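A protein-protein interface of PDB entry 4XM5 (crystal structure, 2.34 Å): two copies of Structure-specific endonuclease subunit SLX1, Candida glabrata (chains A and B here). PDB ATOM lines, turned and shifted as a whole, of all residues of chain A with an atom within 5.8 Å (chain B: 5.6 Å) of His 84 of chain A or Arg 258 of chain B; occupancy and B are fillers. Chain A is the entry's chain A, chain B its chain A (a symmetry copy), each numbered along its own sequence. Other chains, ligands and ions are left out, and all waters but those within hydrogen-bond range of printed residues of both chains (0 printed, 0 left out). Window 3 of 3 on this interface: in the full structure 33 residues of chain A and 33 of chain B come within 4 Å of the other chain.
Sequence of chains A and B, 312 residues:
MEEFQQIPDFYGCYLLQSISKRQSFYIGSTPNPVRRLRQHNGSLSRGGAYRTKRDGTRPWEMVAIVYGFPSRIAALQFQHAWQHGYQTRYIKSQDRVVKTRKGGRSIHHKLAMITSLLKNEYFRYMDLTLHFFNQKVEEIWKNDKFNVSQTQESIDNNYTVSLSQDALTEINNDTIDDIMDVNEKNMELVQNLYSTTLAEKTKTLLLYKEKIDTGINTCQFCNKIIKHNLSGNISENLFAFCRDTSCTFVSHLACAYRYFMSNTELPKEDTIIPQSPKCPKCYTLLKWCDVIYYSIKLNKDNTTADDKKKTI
The backbone carbonyl oxygen (O) of Met 261 of chain B is in hydrogen-bond range of the side-chain hydroxyl (OH) of Tyr 86 of chain A, 3.1 Å away.
Of the printed residues of chain B, Ala 81 of chain A touches Tyr 257.
Of chain B, only Tyr 257 (3.8 Å) and Arg 258 (3.6 Å) come within 4 Å of His 84 of chain A.
Gly 85 of chain A touches none of the printed residues of chain B.
Of the printed residues of chain B, Tyr 86 of chain A touches Met 261 (3.1 Å).
Of the printed residues of chain A, Leu 253 of chain B touches His 80 (3.5 Å).
Of chain A, only His 84 comes within 4 Å of Arg 258 of chain B.
Ser 262 of chain B touches none of the printed residues of chain A.
The nearest printed residue of chain B that does not touch His 84 of chain A is Ala 254 of chain B (4.1 Å).
The nearest residue of chain A that does not touch Arg 258 of chain B is Lys 102 of chain A (4.6 Å).
The nearest printed residue of chain B that does not touch His 80 of chain A is Ala 254 of chain B (4.2 Å).
The backbone carbonyl oxygen (O) of Arg 258 of chain B is in hydrogen-bond range of the side-chain hydroxyl (OG) of Ser 262 of chain B (2.9 Å).
Of the 9 printed residues of chain A, 4 touch a printed residue of chain B.
Hydrophobic or aromatic side chains of chain A within 4 Å of the printed part of chain B: His 80, Ala 81, His 84 and Tyr 86.
Among the printed residues, no Asp or Glu carboxylate lies within 4 Å of a Lys or Arg side-chain nitrogen of the other chain.
His 80 of chain A touches Leu 253 of chain B (CE1 to CD2, 3.5 Å).
O of His 80 of chain A touches CE2 of Tyr 257 of chain B (3.3 Å).
CA of Ala 81 of chain A touches OH of Tyr 257 of chain B, at 3.3 Å.
CE2 of Tyr 257 of chain B touches CB of His 84 of chain A, 3.8 Å away.
His 84 of chain A touches Arg 258 of chain B.
No position is printed for both chains.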
ATOM      1  N   GLN A  79       3.549  32.126  17.637  1.00  0.00           N
ATOM      2  CA  GLN A  79       2.392  32.501  16.825  1.00  0.00           C
ATOM      3  C   GLN A  79       1.746  31.325  16.083  1.00  0.00           C
ATOM      4  O   GLN A  79       0.535  31.112  16.191  1.00  0.00           O
ATOM      5  CB  GLN A  79       2.793  33.558  15.809  1.00  0.00           C
ATOM      6  CG  GLN A  79       1.662  34.056  14.948  1.00  0.00           C
ATOM      7  CD  GLN A  79       2.186  34.696  13.680  1.00  0.00           C
ATOM      8  OE1 GLN A  79       2.981  35.649  13.719  1.00  0.00           O
ATOM      9  NE2 GLN A  79       1.775  34.160  12.544  1.00  0.00           N
ATOM     10  N   HIS A  80       2.547  30.585  15.316  1.00  0.00           N
ATOM     11  CA  HIS A  80       2.019  29.427  14.617  1.00  0.00           C
ATOM     12  C   HIS A  80       1.321  28.485  15.594  1.00  0.00           C
ATOM     13  O   HIS A  80       0.197  28.036  15.329  1.00  0.00           O
ATOM     14  CB  HIS A  80       3.120  28.652  13.852  1.00  0.00           C
ATOM     15  CG  HIS A  80       3.577  29.328  12.599  1.00  0.00           C
ATOM     16  ND1 HIS A  80       4.739  28.970  11.944  1.00  0.00           N
ATOM     17  CD2 HIS A  80       3.036  30.338  11.877  1.00  0.00           C
ATOM     18  CE1 HIS A  80       4.892  29.730  10.875  1.00  0.00           C
ATOM     19  NE2 HIS A  80       3.870  30.567  10.805  1.00  0.00           N
ATOM     20  N   ALA A  81       1.992  28.164  16.701  1.00  0.00           N
ATOM     21  CA  ALA A  81       1.444  27.183  17.624  1.00  0.00           C
ATOM     22  C   ALA A  81       0.154  27.736  18.274  1.00  0.00           C
ATOM     23  O   ALA A  81      -0.821  27.021  18.461  1.00  0.00           O
ATOM     24  CB  ALA A  81       2.461  26.821  18.671  1.00  0.00           C
ATOM     25  N   TRP A  82       0.168  29.015  18.609  1.00  0.00           N
ATOM     26  CA  TRP A  82      -0.979  29.655  19.230  1.00  0.00           C
ATOM     27  C   TRP A  82      -2.179  29.516  18.289  1.00  0.00           C
ATOM     28  O   TRP A  82      -3.238  29.036  18.679  1.00  0.00           O
ATOM     29  CB  TRP A  82      -0.659  31.126  19.529  1.00  0.00           C
ATOM     30  CG  TRP A  82      -1.615  31.807  20.454  1.00  0.00           C
ATOM     31  CD1 TRP A  82      -2.819  31.328  20.919  1.00  0.00           C
ATOM     32  CD2 TRP A  82      -1.448  33.105  21.041  1.00  0.00           C
ATOM     33  NE1 TRP A  82      -3.400  32.253  21.756  1.00  0.00           N
ATOM     34  CE2 TRP A  82      -2.581  33.348  21.851  1.00  0.00           C
ATOM     35  CE3 TRP A  82      -0.454  34.085  20.957  1.00  0.00           C
ATOM     36  CZ2 TRP A  82      -2.749  34.535  22.560  1.00  0.00           C
ATOM     37  CZ3 TRP A  82      -0.605  35.254  21.676  1.00  0.00           C
ATOM     38  CH2 TRP A  82      -1.749  35.471  22.474  1.00  0.00           C
ATOM     39  N   GLN A  83      -1.970  29.870  17.029  1.00  0.00           N
ATOM     40  CA  GLN A  83      -3.013  29.831  16.019  1.00  0.00           C
ATOM     41  C   GLN A  83      -3.537  28.440  15.703  1.00  0.00           C
ATOM     42  O   GLN A  83      -4.746  28.280  15.531  1.00  0.00           O
ATOM     43  CB  GLN A  83      -2.507  30.464  14.725  1.00  0.00           C
ATOM     44  CG  GLN A  83      -2.210  31.931  14.806  1.00  0.00           C
ATOM     45  CD  GLN A  83      -1.668  32.481  13.498  1.00  0.00           C
ATOM     46  OE1 GLN A  83      -0.694  31.963  12.949  1.00  0.00           O
ATOM     47  NE2 GLN A  83      -2.300  33.535  12.986  1.00  0.00           N
ATOM     48  N   HIS A  84      -2.644  27.450  15.611  1.00  0.00           N
ATOM     49  CA  HIS A  84      -2.995  26.116  15.090  1.00  0.00           C
ATOM     50  C   HIS A  84      -2.395  24.942  15.869  1.00  0.00           C
ATOM     51  O   HIS A  84      -2.441  23.803  15.400  1.00  0.00           O
ATOM     52  CB  HIS A  84      -2.546  25.964  13.634  1.00  0.00           C
ATOM     53  CG  HIS A  84      -3.079  27.013  12.715  1.00  0.00           C
ATOM     54  ND1 HIS A  84      -4.416  27.108  12.392  1.00  0.00           N
ATOM     55  CD2 HIS A  84      -2.458  28.012  12.046  1.00  0.00           C
ATOM     56  CE1 HIS A  84      -4.595  28.124  11.567  1.00  0.00           C
ATOM     57  NE2 HIS A  84      -3.423  28.689  11.341  1.00  0.00           N
ATOM     58  N   GLY A  85      -1.815  25.217  17.037  1.00  0.00           N
ATOM     59  CA  GLY A  85      -1.231  24.169  17.855  1.00  0.00           C
ATOM     60  C   GLY A  85      -2.232  23.515  18.783  1.00  0.00           C
ATOM     61  O   GLY A  85      -3.388  23.935  18.876  1.00  0.00           O
ATOM     62  N   TYR A  86      -1.777  22.473  19.470  1.00  0.00           N
ATOM     63  CA  TYR A  86      -2.635  21.669  20.324  1.00  0.00           C
ATOM     64  C   TYR A  86      -2.513  22.082  21.783  1.00  0.00           C
ATOM     65  O   TYR A  86      -1.434  22.468  22.237  1.00  0.00           O
ATOM     66  CB  TYR A  86      -2.289  20.181  20.178  1.00  0.00           C
ATOM     67  CG  TYR A  86      -2.778  19.552  18.896  1.00  0.00           C
ATOM     68  CD1 TYR A  86      -3.734  20.186  18.110  1.00  0.00           C
ATOM     69  CD2 TYR A  86      -2.293  18.319  18.473  1.00  0.00           C
ATOM     70  CE1 TYR A  86      -4.190  19.614  16.936  1.00  0.00           C
ATOM     71  CE2 TYR A  86      -2.741  17.742  17.302  1.00  0.00           C
ATOM     72  CZ  TYR A  86      -3.690  18.395  16.537  1.00  0.00           C
ATOM     73  OH  TYR A  86      -4.144  17.826  15.366  1.00  0.00           O
ATOM     74  N   LYS A 102      -7.385  20.365  19.880  1.00  0.00           N
ATOM     75  CA  LYS A 102      -6.856  21.529  19.182  1.00  0.00           C
ATOM     76  C   LYS A 102      -7.518  22.799  19.714  1.00  0.00           C
ATOM     77  O   LYS A 102      -8.653  22.755  20.204  1.00  0.00           O
ATOM     78  CB  LYS A 102      -7.082  21.390  17.671  1.00  0.00           C
ATOM     79  CG  LYS A 102      -6.397  22.441  16.805  1.00  0.00           C
ATOM     80  CD  LYS A 102      -6.299  21.974  15.354  1.00  0.00           C
ATOM     81  CE  LYS A 102      -5.777  23.068  14.429  1.00  0.00           C
ATOM     82  NZ  LYS A 102      -6.814  24.089  14.103  1.00  0.00           N
ATOM     83  N   LEU B 253       2.997  29.651   4.360  1.00  0.00           N
ATOM     84  CA  LEU B 253       3.740  29.024   5.452  1.00  0.00           C
ATOM     85  C   LEU B 253       2.798  28.596   6.587  1.00  0.00           C
ATOM     86  O   LEU B 253       2.892  27.476   7.097  1.00  0.00           O
ATOM     87  CB  LEU B 253       4.823  29.961   5.992  1.00  0.00           C
ATOM     88  CG  LEU B 253       5.703  29.330   7.079  1.00  0.00           C
ATOM     89  CD1 LEU B 253       6.615  28.224   6.539  1.00  0.00           C
ATOM     90  CD2 LEU B 253       6.548  30.381   7.808  1.00  0.00           C
ATOM     91  N   ALA B 254       1.865  29.471   6.963  1.00  0.00           N
ATOM     92  CA  ALA B 254       0.975  29.152   8.075  1.00  0.00           C
ATOM     93  C   ALA B 254       0.003  28.030   7.707  1.00  0.00           C
ATOM     94  O   ALA B 254      -0.382  27.234   8.556  1.00  0.00           O
ATOM     95  CB  ALA B 254       0.224  30.388   8.533  1.00  0.00           C
ATOM     96  N   CYS B 255      -0.381  27.947   6.440  1.00  0.00           N
ATOM     97  CA  CYS B 255      -1.227  26.838   5.989  1.00  0.00           C
ATOM     98  C   CYS B 255      -0.521  25.493   6.048  1.00  0.00           C
ATOM     99  O   CYS B 255      -1.118  24.477   6.427  1.00  0.00           O
ATOM    100  CB  CYS B 255      -1.702  27.081   4.575  1.00  0.00           C
ATOM    101  SG  CYS B 255      -2.889  28.375   4.533  1.00  0.00           S
ATOM    102  N   ALA B 256       0.748  25.488   5.651  1.00  0.00           N
ATOM    103  CA  ALA B 256       1.522  24.261   5.656  1.00  0.00           C
ATOM    104  C   ALA B 256       1.617  23.763   7.083  1.00  0.00           C
ATOM    105  O   ALA B 256       1.417  22.579   7.356  1.00  0.00           O
ATOM    106  CB  ALA B 256       2.921  24.479   5.054  1.00  0.00           C
ATOM    107  N   TYR B 257       1.901  24.686   7.994  1.00  0.00           N
ATOM    108  CA  TYR B 257       2.054  24.345   9.396  1.00  0.00           C
ATOM    109  C   TYR B 257       0.779  23.692   9.927  1.00  0.00           C
ATOM    110  O   TYR B 257       0.825  22.716  10.681  1.00  0.00           O
ATOM    111  CB  TYR B 257       2.394  25.588  10.212  1.00  0.00           C
ATOM    112  CG  TYR B 257       2.368  25.338  11.701  1.00  0.00           C
ATOM    113  CD1 TYR B 257       3.511  24.895  12.359  1.00  0.00           C
ATOM    114  CD2 TYR B 257       1.205  25.527  12.445  1.00  0.00           C
ATOM    115  CE1 TYR B 257       3.498  24.646  13.714  1.00  0.00           C
ATOM    116  CE2 TYR B 257       1.184  25.267  13.806  1.00  0.00           C
ATOM    117  CZ  TYR B 257       2.348  24.841  14.426  1.00  0.00           C
ATOM    118  OH  TYR B 257       2.370  24.575  15.762  1.00  0.00           O
ATOM    119  N   ARG B 258      -0.356  24.257   9.532  1.00  0.00           N
ATOM    120  CA  ARG B 258      -1.652  23.780   9.959  1.00  0.00           C
ATOM    121  C   ARG B 258      -1.880  22.366   9.428  1.00  0.00           C
ATOM    122  O   ARG B 258      -2.275  21.457  10.174  1.00  0.00           O
ATOM    123  CB  ARG B 258      -2.741  24.738   9.468  1.00  0.00           C
ATOM    124  CG  ARG B 258      -4.134  24.442   9.963  1.00  0.00           C
ATOM    125  CD  ARG B 258      -5.133  25.326   9.238  1.00  0.00           C
ATOM    126  NE  ARG B 258      -6.511  25.000   9.588  1.00  0.00           N
ATOM    127  N   TYR B 259      -1.620  22.176   8.137  1.00  0.00           N
ATOM    128  CA  TYR B 259      -1.758  20.853   7.567  1.00  0.00           C
ATOM    129  C   TYR B 259      -0.832  19.889   8.288  1.00  0.00           C
ATOM    130  O   TYR B 259      -1.265  18.842   8.770  1.00  0.00           O
ATOM    131  CB  TYR B 259      -1.463  20.834   6.069  1.00  0.00           C
ATOM    132  CG  TYR B 259      -1.482  19.424   5.546  1.00  0.00           C
ATOM    133  CD1 TYR B 259      -2.681  18.728   5.420  1.00  0.00           C
ATOM    134  CD2 TYR B 259      -0.302  18.766   5.221  1.00  0.00           C
ATOM    135  CE1 TYR B 259      -2.708  17.426   4.963  1.00  0.00           C
ATOM    136  CE2 TYR B 259      -0.322  17.461   4.757  1.00  0.00           C
ATOM    137  CZ  TYR B 259      -1.527  16.801   4.634  1.00  0.00           C
ATOM    138  OH  TYR B 259      -1.537  15.507   4.177  1.00  0.00           O
ATOM    139  N   PHE B 260       0.435  20.261   8.387  1.00  0.00           N
ATOM    140  CA  PHE B 260       1.433  19.413   9.036  1.00  0.00           C
ATOM    141  C   PHE B 260       1.073  19.038  10.472  1.00  0.00           C
ATOM    142  O   PHE B 260       1.380  17.922  10.901  1.00  0.00           O
ATOM    143  CB  PHE B 260       2.809  20.092   8.989  1.00  0.00           C
ATOM    144  CG  PHE B 260       3.407  20.128   7.604  1.00  0.00           C
ATOM    145  CD1 PHE B 260       3.184  19.080   6.722  1.00  0.00           C
ATOM    146  CD2 PHE B 260       4.159  21.206   7.174  1.00  0.00           C
ATOM    147  CE1 PHE B 260       3.720  19.106   5.435  1.00  0.00           C
ATOM    148  CE2 PHE B 260       4.690  21.244   5.891  1.00  0.00           C
ATOM    149  CZ  PHE B 260       4.474  20.195   5.025  1.00  0.00           C
ATOM    150  N   MET B 261       0.416  19.944  11.203  1.00  0.00           N
ATOM    151  CA  MET B 261       0.037  19.664  12.592  1.00  0.00           C
ATOM    152  C   MET B 261      -1.219  18.818  12.648  1.00  0.00           C
ATOM    153  O   MET B 261      -1.590  18.338  13.713  1.00  0.00           O
ATOM    154  CB  MET B 261      -0.190  20.953  13.417  1.00  0.00           C
ATOM    155  CG  MET B 261       1.069  21.709  13.826  1.00  0.00           C
ATOM    156  SD  MET B 261       2.387  20.716  14.565  1.00  0.00           S
ATOM    157  CE  MET B 261       1.599  20.124  16.037  1.00  0.00           C
ATOM    158  N   SER B 262      -1.868  18.637  11.503  1.00  0.00           N
ATOM    159  CA  SER B 262      -3.083  17.828  11.430  1.00  0.00           C
ATOM    160  C   SER B 262      -2.802  16.359  11.125  1.00  0.00           C
ATOM    161  O   SER B 262      -3.310  15.469  11.805  1.00  0.00           O
ATOM    162  CB  SER B 262      -4.033  18.397  10.378  1.00  0.00           C
ATOM    163  OG  SER B 262      -4.481  19.688  10.751  1.00  0.00           O
ATOM    164  N   ASN B 263      -1.998  16.108  10.099  1.00  0.00           N
ATOM    165  CA  ASN B 263      -1.740  14.744   9.651  1.00  0.00           C
ATOM    166  C   ASN B 263      -0.251  14.465   9.424  1.00  0.00           C
ATOM    167  O   ASN B 263       0.542  14.419  10.374  1.00  0.00           O
ATOM    168  CB  ASN B 263      -2.529  14.463   8.372  1.00  0.00           C
